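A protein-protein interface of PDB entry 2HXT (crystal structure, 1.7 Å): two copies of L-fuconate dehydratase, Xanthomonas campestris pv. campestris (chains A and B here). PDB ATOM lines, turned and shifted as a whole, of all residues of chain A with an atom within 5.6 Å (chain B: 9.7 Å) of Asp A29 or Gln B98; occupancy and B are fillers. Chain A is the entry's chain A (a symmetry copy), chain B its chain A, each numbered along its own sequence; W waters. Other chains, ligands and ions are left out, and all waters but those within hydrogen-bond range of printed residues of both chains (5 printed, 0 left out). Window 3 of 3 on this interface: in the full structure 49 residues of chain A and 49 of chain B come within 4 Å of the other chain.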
ATOM      1  N   SER A  17       8.950  32.589 -10.722  1.00  0.00           N
ATOM      2  CA  SER A  17       9.236  31.448 -11.584  1.00  0.00           C
ATOM      3  C   SER A  17      10.704  31.357 -12.005  1.00  0.00           C
ATOM      4  O   SER A  17      11.163  30.301 -12.435  1.00  0.00           O
ATOM      5  CB  SER A  17       8.347  31.491 -12.832  1.00  0.00           C
ATOM      6  OG  SER A  17       8.608  32.646 -13.611  1.00  0.00           O
ATOM      7  N   LEU A  20      11.853  29.094  -9.658  1.00  0.00           N
ATOM      8  CA  LEU A  20      10.812  28.111  -9.388  1.00  0.00           C
ATOM      9  C   LEU A  20      10.322  28.135  -7.945  1.00  0.00           C
ATOM     10  O   LEU A  20       9.928  27.105  -7.396  1.00  0.00           O
ATOM     11  CB  LEU A  20      11.298  26.705  -9.750  1.00  0.00           C
ATOM     12  CG  LEU A  20      11.639  26.489 -11.227  1.00  0.00           C
ATOM     13  CD1 LEU A  20      12.089  25.053 -11.441  1.00  0.00           C
ATOM     14  CD2 LEU A  20      10.423  26.801 -12.088  1.00  0.00           C
ATOM     15  N   SER A  23       6.824  26.508  -6.778  1.00  0.00           N
ATOM     16  CA  SER A  23       6.482  25.424  -7.697  1.00  0.00           C
ATOM     17  C   SER A  23       5.942  24.167  -7.016  1.00  0.00           C
ATOM     18  O   SER A  23       6.392  23.785  -5.936  1.00  0.00           O
ATOM     19  CB  SER A  23       7.703  25.056  -8.548  1.00  0.00           C
ATOM     20  OG  SER A  23       8.808  24.692  -7.734  1.00  0.00           O
ATOM     21  N   ASN A  27       1.113  23.421 -10.264  1.00  0.00           N
ATOM     22  CA  ASN A  27       1.603  24.723 -10.717  1.00  0.00           C
ATOM     23  C   ASN A  27       3.130  24.671 -10.751  1.00  0.00           C
ATOM     24  O   ASN A  27       3.795  24.994  -9.771  1.00  0.00           O
ATOM     25  CB  ASN A  27       1.134  25.801  -9.740  1.00  0.00           C
ATOM     26  CG  ASN A  27      -0.310  25.608  -9.318  1.00  0.00           C
ATOM     27  OD1 ASN A  27      -1.225  25.695 -10.138  1.00  0.00           O
ATOM     28  ND2 ASN A  27      -0.521  25.332  -8.032  1.00  0.00           N
ATOM     29  N   PRO A  28       3.700  24.274 -11.896  1.00  0.00           N
ATOM     30  CA  PRO A  28       5.149  24.155 -12.091  1.00  0.00           C
ATOM     31  C   PRO A  28       5.965  25.441 -12.146  1.00  0.00           C
ATOM     32  O   PRO A  28       7.176  25.410 -11.917  1.00  0.00           O
ATOM     33  CB  PRO A  28       5.260  23.372 -13.401  1.00  0.00           C
ATOM     34  CG  PRO A  28       3.930  22.675 -13.526  1.00  0.00           C
ATOM     35  CD  PRO A  28       2.983  23.740 -13.063  1.00  0.00           C
ATOM     36  N   ASP A  29       5.325  26.565 -12.452  1.00  0.00           N
ATOM     37  CA  ASP A  29       6.063  27.821 -12.561  1.00  0.00           C
ATOM     38  C   ASP A  29       5.245  29.058 -12.213  1.00  0.00           C
ATOM     39  O   ASP A  29       5.152  29.993 -13.008  1.00  0.00           O
ATOM     40  CB  ASP A  29       6.614  27.961 -13.983  1.00  0.00           C
ATOM     41  CG  ASP A  29       5.519  27.948 -15.045  1.00  0.00           C
ATOM     42  OD1 ASP A  29       4.352  27.635 -14.719  1.00  0.00           O
ATOM     43  OD2 ASP A  29       5.830  28.245 -16.217  1.00  0.00           O
ATOM     44  N   PRO A  30       4.663  29.092 -11.007  1.00  0.00           N
ATOM     45  CA  PRO A  30       3.861  30.252 -10.617  1.00  0.00           C
ATOM     46  C   PRO A  30       4.661  31.539 -10.465  1.00  0.00           C
ATOM     47  O   PRO A  30       5.828  31.522 -10.075  1.00  0.00           O
ATOM     48  CB  PRO A  30       3.246  29.813  -9.294  1.00  0.00           C
ATOM     49  CG  PRO A  30       4.341  28.967  -8.703  1.00  0.00           C
ATOM     50  CD  PRO A  30       4.776  28.132  -9.893  1.00  0.00           C
ATOM     51  N   ASP A  31       4.021  32.650 -10.814  1.00  0.00           N
ATOM     52  CA  ASP A  31       4.606  33.971 -10.653  1.00  0.00           C
ATOM     53  C   ASP A  31       3.675  34.615  -9.636  1.00  0.00           C
ATOM     54  O   ASP A  31       2.616  35.135  -9.996  1.00  0.00           O
ATOM     55  CB  ASP A  31       4.578  34.754 -11.969  1.00  0.00           C
ATOM     56  CG  ASP A  31       5.710  34.368 -12.899  1.00  0.00           C
ATOM     57  OD1 ASP A  31       5.471  34.292 -14.121  1.00  0.00           O
ATOM     58  OD2 ASP A  31       6.846  34.156 -12.417  1.00  0.00           O
ATOM     59  N   ILE A  56      -1.369  33.491  -9.335  1.00  0.00           N
ATOM     60  CA  ILE A  56      -0.022  33.081  -9.694  1.00  0.00           C
ATOM     61  C   ILE A  56       0.467  33.495 -11.075  1.00  0.00           C
ATOM     62  O   ILE A  56       1.235  32.776 -11.712  1.00  0.00           O
ATOM     63  CB  ILE A  56       0.159  31.554  -9.507  1.00  0.00           C
ATOM     64  CG1 ILE A  56      -0.945  30.783 -10.231  1.00  0.00           C
ATOM     65  CG2 ILE A  56       0.137  31.222  -8.014  1.00  0.00           C
ATOM     66  CD1 ILE A  56      -0.700  29.277 -10.264  1.00  0.00           C
ATOM     67  N   GLY A  57       0.036  34.669 -11.527  1.00  0.00           N
ATOM     68  CA  GLY A  57       0.501  35.161 -12.814  1.00  0.00           C
ATOM     69  C   GLY A  57      -0.595  35.486 -13.801  1.00  0.00           C
ATOM     70  O   GLY A  57      -1.362  36.431 -13.604  1.00  0.00           O
ATOM     71  N   ARG A  58      -0.663  34.706 -14.872  1.00  0.00           N
ATOM     72  CA  ARG A  58      -1.681  34.921 -15.889  1.00  0.00           C
ATOM     73  C   ARG A  58      -3.050  34.956 -15.227  1.00  0.00           C
ATOM     74  O   ARG A  58      -3.327  34.184 -14.305  1.00  0.00           O
ATOM     75  CB  ARG A  58      -1.619  33.811 -16.938  1.00  0.00           C
ATOM     76  CG  ARG A  58      -0.346  33.841 -17.777  1.00  0.00           C
ATOM     77  CD  ARG A  58      -0.382  32.780 -18.867  1.00  0.00           C
ATOM     78  NE  ARG A  58      -0.377  31.431 -18.311  1.00  0.00           N
ATOM     79  CZ  ARG A  58       0.712  30.792 -17.895  1.00  0.00           C
ATOM     80  NH1 ARG A  58       1.908  31.370 -17.977  1.00  0.00           N
ATOM     81  NH2 ARG A  58       0.602  29.576 -17.375  1.00  0.00           N
ATOM     82  N   GLY A  59      -3.898  35.865 -15.694  1.00  0.00           N
ATOM     83  CA  GLY A  59      -5.222  36.003 -15.125  1.00  0.00           C
ATOM     84  C   GLY A  59      -5.280  37.071 -14.050  1.00  0.00           C
ATOM     85  O   GLY A  59      -6.366  37.496 -13.654  1.00  0.00           O
ATOM     86  N   LEU B  70      -8.245  35.383 -23.110  1.00  0.00           N
ATOM     87  CA  LEU B  70      -7.875  34.094 -23.682  1.00  0.00           C
ATOM     88  C   LEU B  70      -7.327  34.225 -25.101  1.00  0.00           C
ATOM     89  O   LEU B  70      -6.943  33.235 -25.718  1.00  0.00           O
ATOM     90  CB  LEU B  70      -9.087  33.159 -23.674  1.00  0.00           C
ATOM     91  CG  LEU B  70      -9.610  32.813 -22.276  1.00  0.00           C
ATOM     92  CD1 LEU B  70     -10.935  32.074 -22.380  1.00  0.00           C
ATOM     93  CD2 LEU B  70      -8.574  31.966 -21.547  1.00  0.00           C
ATOM     94  N   HIS B  73      -3.860  32.677 -25.941  1.00  0.00           N
ATOM     95  CA  HIS B  73      -3.862  31.229 -26.113  1.00  0.00           C
ATOM     96  C   HIS B  73      -4.414  30.745 -27.449  1.00  0.00           C
ATOM     97  O   HIS B  73      -3.945  29.747 -27.994  1.00  0.00           O
ATOM     98  CB  HIS B  73      -4.692  30.563 -25.009  1.00  0.00           C
ATOM     99  CG  HIS B  73      -3.909  30.185 -23.792  1.00  0.00           C
ATOM    100  ND1 HIS B  73      -2.810  29.353 -23.842  1.00  0.00           N
ATOM    101  CD2 HIS B  73      -4.100  30.476 -22.484  1.00  0.00           C
ATOM    102  CE1 HIS B  73      -2.362  29.146 -22.617  1.00  0.00           C
ATOM    103  NE2 HIS B  73      -3.128  29.815 -21.774  1.00  0.00           N
ATOM    104  N   ARG B  92      -5.693  23.120 -23.496  1.00  0.00           N
ATOM    105  CA  ARG B  92      -4.759  24.237 -23.538  1.00  0.00           C
ATOM    106  C   ARG B  92      -5.229  25.309 -22.561  1.00  0.00           C
ATOM    107  O   ARG B  92      -4.419  26.002 -21.944  1.00  0.00           O
ATOM    108  CB  ARG B  92      -4.683  24.830 -24.951  1.00  0.00           C
ATOM    109  CG  ARG B  92      -3.805  26.070 -25.045  1.00  0.00           C
ATOM    110  CD  ARG B  92      -3.701  26.613 -26.471  1.00  0.00           C
ATOM    111  NE  ARG B  92      -3.026  25.683 -27.374  1.00  0.00           N
ATOM    112  CZ  ARG B  92      -3.652  24.862 -28.213  1.00  0.00           C
ATOM    113  NH1 ARG B  92      -2.952  24.049 -28.993  1.00  0.00           N
ATOM    114  NH2 ARG B  92      -4.974  24.864 -28.285  1.00  0.00           N
ATOM    115  N   LEU B  93      -6.544  25.424 -22.415  1.00  0.00           N
ATOM    116  CA  LEU B  93      -7.129  26.420 -21.530  1.00  0.00           C
ATOM    117  C   LEU B  93      -7.366  25.906 -20.112  1.00  0.00           C
ATOM    118  O   LEU B  93      -6.978  26.554 -19.139  1.00  0.00           O
ATOM    119  CB  LEU B  93      -8.449  26.924 -22.128  1.00  0.00           C
ATOM    120  CG  LEU B  93      -8.393  27.336 -23.605  1.00  0.00           C
ATOM    121  CD1 LEU B  93      -9.771  27.789 -24.070  1.00  0.00           C
ATOM    122  CD2 LEU B  93      -7.382  28.454 -23.793  1.00  0.00           C
ATOM    123  N   THR B  94      -7.989  24.739 -19.983  1.00  0.00           N
ATOM    124  CA  THR B  94      -8.265  24.213 -18.652  1.00  0.00           C
ATOM    125  C   THR B  94      -7.026  23.752 -17.899  1.00  0.00           C
ATOM    126  O   THR B  94      -7.031  23.719 -16.667  1.00  0.00           O
ATOM    127  CB  THR B  94      -9.298  23.062 -18.692  1.00  0.00           C
ATOM    128  OG1 THR B  94      -8.835  22.014 -19.551  1.00  0.00           O
ATOM    129  CG2 THR B  94     -10.637  23.583 -19.195  1.00  0.00           C
ATOM    130  N   ASN B  95      -5.963  23.408 -18.622  1.00  0.00           N
ATOM    131  CA  ASN B  95      -4.735  22.969 -17.968  1.00  0.00           C
ATOM    132  C   ASN B  95      -3.709  24.082 -17.778  1.00  0.00           C
ATOM    133  O   ASN B  95      -2.566  23.814 -17.417  1.00  0.00           O
ATOM    134  CB  ASN B  95      -4.093  21.794 -18.712  1.00  0.00           C
ATOM    135  CG  ASN B  95      -4.838  20.492 -18.493  1.00  0.00           C
ATOM    136  OD1 ASN B  95      -5.470  20.295 -17.456  1.00  0.00           O
ATOM    137  ND2 ASN B  95      -4.756  19.588 -19.463  1.00  0.00           N
ATOM    138  N   ASP B  96      -4.106  25.324 -18.041  1.00  0.00           N
ATOM    139  CA  ASP B  96      -3.209  26.456 -17.812  1.00  0.00           C
ATOM    140  C   ASP B  96      -3.306  26.605 -16.297  1.00  0.00           C
ATOM    141  O   ASP B  96      -4.307  27.110 -15.789  1.00  0.00           O
ATOM    142  CB  ASP B  96      -3.738  27.723 -18.490  1.00  0.00           C
ATOM    143  CG  ASP B  96      -2.852  28.933 -18.235  1.00  0.00           C
ATOM    144  OD1 ASP B  96      -2.299  29.037 -17.122  1.00  0.00           O
ATOM    145  OD2 ASP B  96      -2.723  29.791 -19.135  1.00  0.00           O
ATOM    146  N   SER B  97      -2.281  26.155 -15.575  1.00  0.00           N
ATOM    147  CA  SER B  97      -2.308  26.204 -14.114  1.00  0.00           C
ATOM    148  C   SER B  97      -2.548  27.581 -13.511  1.00  0.00           C
ATOM    149  O   SER B  97      -3.159  27.702 -12.448  1.00  0.00           O
ATOM    150  CB  SER B  97      -1.021  25.599 -13.535  1.00  0.00           C
ATOM    151  OG  SER B  97       0.121  26.318 -13.954  1.00  0.00           O
ATOM    152  N   GLN B  98      -2.081  28.627 -14.179  1.00  0.00           N
ATOM    153  CA  GLN B  98      -2.282  29.961 -13.645  1.00  0.00           C
ATOM    154  C   GLN B  98      -3.745  30.386 -13.776  1.00  0.00           C
ATOM    155  O   GLN B  98      -4.283  31.052 -12.892  1.00  0.00           O
ATOM    156  CB  GLN B  98      -1.293  30.923 -14.314  1.00  0.00           C
ATOM    157  CG  GLN B  98       0.119  30.653 -13.781  1.00  0.00           C
ATOM    158  CD  GLN B  98       1.224  31.401 -14.499  1.00  0.00           C
ATOM    159  OE1 GLN B  98       1.028  32.504 -14.999  1.00  0.00           O
ATOM    160  NE2 GLN B  98       2.412  30.804 -14.521  1.00  0.00           N
ATOM    161  N   LEU B  99      -4.407  29.969 -14.849  1.00  0.00           N
ATOM    162  CA  LEU B  99      -5.823  30.294 -14.993  1.00  0.00           C
ATOM    163  C   LEU B  99      -6.619  29.402 -14.033  1.00  0.00           C
ATOM    164  O   LEU B  99      -7.676  29.799 -13.537  1.00  0.00           O
ATOM    165  CB  LEU B  99      -6.299  30.076 -16.436  1.00  0.00           C
ATOM    166  CG  LEU B  99      -5.684  31.010 -17.484  1.00  0.00           C
ATOM    167  CD1 LEU B  99      -6.375  30.786 -18.823  1.00  0.00           C
ATOM    168  CD2 LEU B  99      -5.844  32.465 -17.052  1.00  0.00           C
ATOM    169  N   ARG B 100      -6.112  28.199 -13.765  1.00  0.00           N
ATOM    170  CA  ARG B 100      -6.803  27.295 -12.846  1.00  0.00           C
ATOM    171  C   ARG B 100      -6.879  27.921 -11.460  1.00  0.00           C
ATOM    172  O   ARG B 100      -7.847  27.723 -10.736  1.00  0.00           O
ATOM    173  CB  ARG B 100      -6.088  25.939 -12.728  1.00  0.00           C
ATOM    174  CG  ARG B 100      -6.192  25.022 -13.941  1.00  0.00           C
ATOM    175  CD  ARG B 100      -5.651  23.623 -13.615  1.00  0.00           C
ATOM    176  NE  ARG B 100      -6.517  22.891 -12.687  1.00  0.00           N
ATOM    177  CZ  ARG B 100      -7.647  22.284 -13.041  1.00  0.00           C
ATOM    178  NH1 ARG B 100      -8.048  22.311 -14.305  1.00  0.00           N
ATOM    179  NH2 ARG B 100      -8.390  21.665 -12.130  1.00  0.00           N
ATOM    180  N   TRP B 101      -5.856  28.683 -11.091  1.00  0.00           N
ATOM    181  CA  TRP B 101      -5.836  29.305  -9.775  1.00  0.00           C
ATOM    182  C   TRP B 101      -7.048  30.206  -9.546  1.00  0.00           C
ATOM    183  O   TRP B 101      -7.520  30.344  -8.416  1.00  0.00           O
ATOM    184  CB  TRP B 101      -4.543  30.108  -9.585  1.00  0.00           C
ATOM    185  CG  TRP B 101      -4.330  30.522  -8.165  1.00  0.00           C
ATOM    186  CD1 TRP B 101      -4.785  31.660  -7.561  1.00  0.00           C
ATOM    187  CD2 TRP B 101      -3.667  29.764  -7.148  1.00  0.00           C
ATOM    188  NE1 TRP B 101      -4.448  31.655  -6.226  1.00  0.00           N
ATOM    189  CE2 TRP B 101      -3.763  30.502  -5.946  1.00  0.00           C
ATOM    190  CE3 TRP B 101      -3.001  28.529  -7.134  1.00  0.00           C
ATOM    191  CZ2 TRP B 101      -3.220  30.044  -4.740  1.00  0.00           C
ATOM    192  CZ3 TRP B 101      -2.459  28.073  -5.930  1.00  0.00           C
ATOM    193  CH2 TRP B 101      -2.575  28.832  -4.753  1.00  0.00           C
ATOM    194  N   LEU B 102      -7.552  30.813 -10.620  1.00  0.00           N
ATOM    195  CA  LEU B 102      -8.707  31.702 -10.528  1.00  0.00           C
ATOM    196  C   LEU B 102     -10.012  30.937 -10.327  1.00  0.00           C
ATOM    197  O   LEU B 102     -11.070  31.537 -10.121  1.00  0.00           O
ATOM    198  CB  LEU B 102      -8.808  32.577 -11.783  1.00  0.00           C
ATOM    199  CG  LEU B 102      -7.944  33.841 -11.829  1.00  0.00           C
ATOM    200  CD1 LEU B 102      -6.478  33.504 -11.629  1.00  0.00           C
ATOM    201  CD2 LEU B 102      -8.160  34.535 -13.163  1.00  0.00           C
ATOM    202  N   GLY B 103      -9.919  29.613 -10.386  1.00  0.00           N
ATOM    203  CA  GLY B 103     -11.080  28.764 -10.188  1.00  0.00           C
ATOM    204  C   GLY B 103     -10.805  27.868  -8.995  1.00  0.00           C
ATOM    205  O   GLY B 103     -10.932  28.313  -7.854  1.00  0.00           O
ATOM    206  N   PRO B 104     -10.420  26.601  -9.220  1.00  0.00           N
ATOM    207  CA  PRO B 104     -10.249  25.980 -10.541  1.00  0.00           C
ATOM    208  C   PRO B 104     -11.577  25.451 -11.072  1.00  0.00           C
ATOM    209  O   PRO B 104     -12.414  24.984 -10.305  1.00  0.00           O
ATOM    210  CB  PRO B 104      -9.271  24.827 -10.276  1.00  0.00           C
ATOM    211  CG  PRO B 104      -8.713  25.099  -8.884  1.00  0.00           C
ATOM    212  CD  PRO B 104      -9.864  25.736  -8.169  1.00  0.00           C
ATOM    213  N   GLU B 105     -11.761  25.524 -12.385  1.00  0.00           N
ATOM    214  CA  GLU B 105     -12.970  25.021 -13.020  1.00  0.00           C
ATOM    215  C   GLU B 105     -14.269  25.481 -12.358  1.00  0.00           C
ATOM    216  O   GLU B 105     -15.161  24.677 -12.075  1.00  0.00           O
ATOM    217  CB  GLU B 105     -12.915  23.490 -13.080  1.00  0.00           C
ATOM    218  CG  GLU B 105     -11.619  22.971 -13.691  1.00  0.00           C
ATOM    219  CD  GLU B 105     -11.588  21.462 -13.850  1.00  0.00           C
ATOM    220  OE1 GLU B 105     -10.473  20.902 -13.942  1.00  0.00           O
ATOM    221  OE2 GLU B 105     -12.668  20.836 -13.893  1.00  0.00           O
ATOM    222  N   MET B 109     -13.643  32.749 -14.612  1.00  0.00           N
ATOM    223  CA  MET B 109     -12.599  32.259 -15.506  1.00  0.00           C
ATOM    224  C   MET B 109     -12.980  30.974 -16.229  1.00  0.00           C
ATOM    225  O   MET B 109     -12.659  30.807 -17.404  1.00  0.00           O
ATOM    226  CB  MET B 109     -11.279  32.073 -14.751  1.00  0.00           C
ATOM    227  CG  MET B 109     -10.038  32.129 -15.652  1.00  0.00           C
ATOM    228  SD  MET B 109      -9.764  33.746 -16.471  1.00  0.00           S
ATOM    229  CE  MET B 109     -10.142  33.335 -18.176  1.00  0.00           C
ATOM    230  N   ILE B 113     -13.596  30.344 -20.309  1.00  0.00           N
ATOM    231  CA  ILE B 113     -12.945  29.256 -21.024  1.00  0.00           C
ATOM    232  C   ILE B 113     -14.000  28.411 -21.741  1.00  0.00           C
ATOM    233  O   ILE B 113     -13.804  27.994 -22.884  1.00  0.00           O
ATOM    234  CB  ILE B 113     -12.122  28.387 -20.041  1.00  0.00           C
ATOM    235  CG1 ILE B 113     -10.854  29.151 -19.638  1.00  0.00           C
ATOM    236  CG2 ILE B 113     -11.776  27.044 -20.669  1.00  0.00           C
ATOM    237  CD1 ILE B 113     -10.077  28.519 -18.503  1.00  0.00           C
HETATM  238  O   HOH W   1       5.433  31.606 -15.183  1.00  0.00           O
HETATM  239  O   HOH W   2       3.051  34.320 -15.472  1.00  0.00           O
HETATM  240  O   HOH W   3      -3.098  33.117 -11.628  1.00  0.00           O
HETATM  241  O   HOH W   4      -3.905  25.882  -9.812  1.00  0.00           O
HETATM  242  O   HOH W   5       2.361  27.724 -12.855  1.00  0.00           O
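Water W3 lies within hydrogen-bond range of O of Gln B98 (2.7 Å), O of Arg A58 (2.9 Å), N of Ile A56 (2.9 Å) and N of Gly A57 (3.5 Å). Water W4 bridges the side-chain amide oxygen (OD1) of Asn A27 and the backbone carbonyl oxygen (O) of Ser B97. Water W1 lies within hydrogen-bond range of the backbone carbonyl oxygen (O) of Asp A29 (2.7 Å), the side-chain carboxylate (OD1) of Asp A31 (2.9 Å) and the side-chain amide nitrogen (NE2) of Gln B98 (3.2 Å). Water W5 lies within hydrogen-bond range of the side-chain carboxylate of Asp A29 and the side-chain hydroxyl of Ser B97. Water W2 bridges OE1 of Gln B98 (2.8 Å) and OD1 of Asp A31 (2.8 Å).
Of the 12 printed residues of chain A, 7 touch a printed residue of chain B. Printed residues of chain A that touch a printed residue of chain B: Asn A27, Pro A28, Asp A29, Ile A56, Gly A57, Arg A58 and Gly A59. Hydrophobic or aromatic side chains of chain A that line the printed part of chain B: Pro A28 and Ile A56. Of the 18 printed residues of chain B, 5 touch a printed residue of chain A. Hydrophobic or aromatic side chains of chain B within 4 Å of the printed part of chain A: Trp B101 and Leu B102.
NH2 of Arg A58 is in salt-bridge range of OD1 of Asp B96, at 3.0 Å. NE2 of Gln B98 sits at hydrogen-bond distance from O of Asp A29, at 3.2 Å. The side-chain amide oxygen of Gln B98 lies close to the backbone carbonyl oxygen of Ile A56 (3.3 Å). N of Arg A58 sits at hydrogen-bond distance from OE1 of Gln B98, 2.8 Å away.
Printed residues of chain B within 4 Å of Asn A27: Ser B97 and Trp B101. Asp A29 touches just one residue of chain B: Gln B98 (3.2 Å). Asp A31 touches none of the printed residues of chain B. Printed residues of chain B within 4 Å of Arg A58: Asp B96 (3.0 Å) and Gln B98 (2.8 Å). Leu B70 touches none of the printed residues of chain A. Of the printed residues of chain A, Asp B96 touches Arg A58. Of the printed residues of chain A, Trp B101 touches Asn A27 (3.96 Å) and Ile A56 (3.7 Å). The nearest residue of chain B that does not touch Asp A29 is Ser B97 (4.5 Å). The nearest residue of chain A that does not touch Gln B98 is Pro A30 (4.2 Å).
The side-chain carboxylate of Asp B96 is in hydrogen-bond range of a ring nitrogen (NE2) of His B73 (2.7 Å). The backbone NH of Gln B98 lies within hydrogen-bond range of the side-chain carboxylate of Asp B96 (3.0 Å). OD1 of Asp B96 sits at hydrogen-bond distance from N of Leu B99 (3.2 Å). N of Asp A31 sits at hydrogen-bond distance from O of Ile A56. The backbone carbonyl oxygen of Asp A31 is in hydrogen-bond range of the backbone NH of Gly A57 (3.0 Å).
Among the printed residues, pairs that only touch across the chains: Asn A27 with Ser B97 (3.4 Å), Gly A57 with Gln B98 (3.5 Å), Gly A59 with Leu B102 (3.5 Å), Ile A56 with Ser B97 (3.6 Å), Ile A56 with Trp B101 (3.7 Å), Pro A28 with Ser B97 (3.95 Å) and Asn A27 with Trp B101 (3.96 Å).
No position is printed for both chains.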
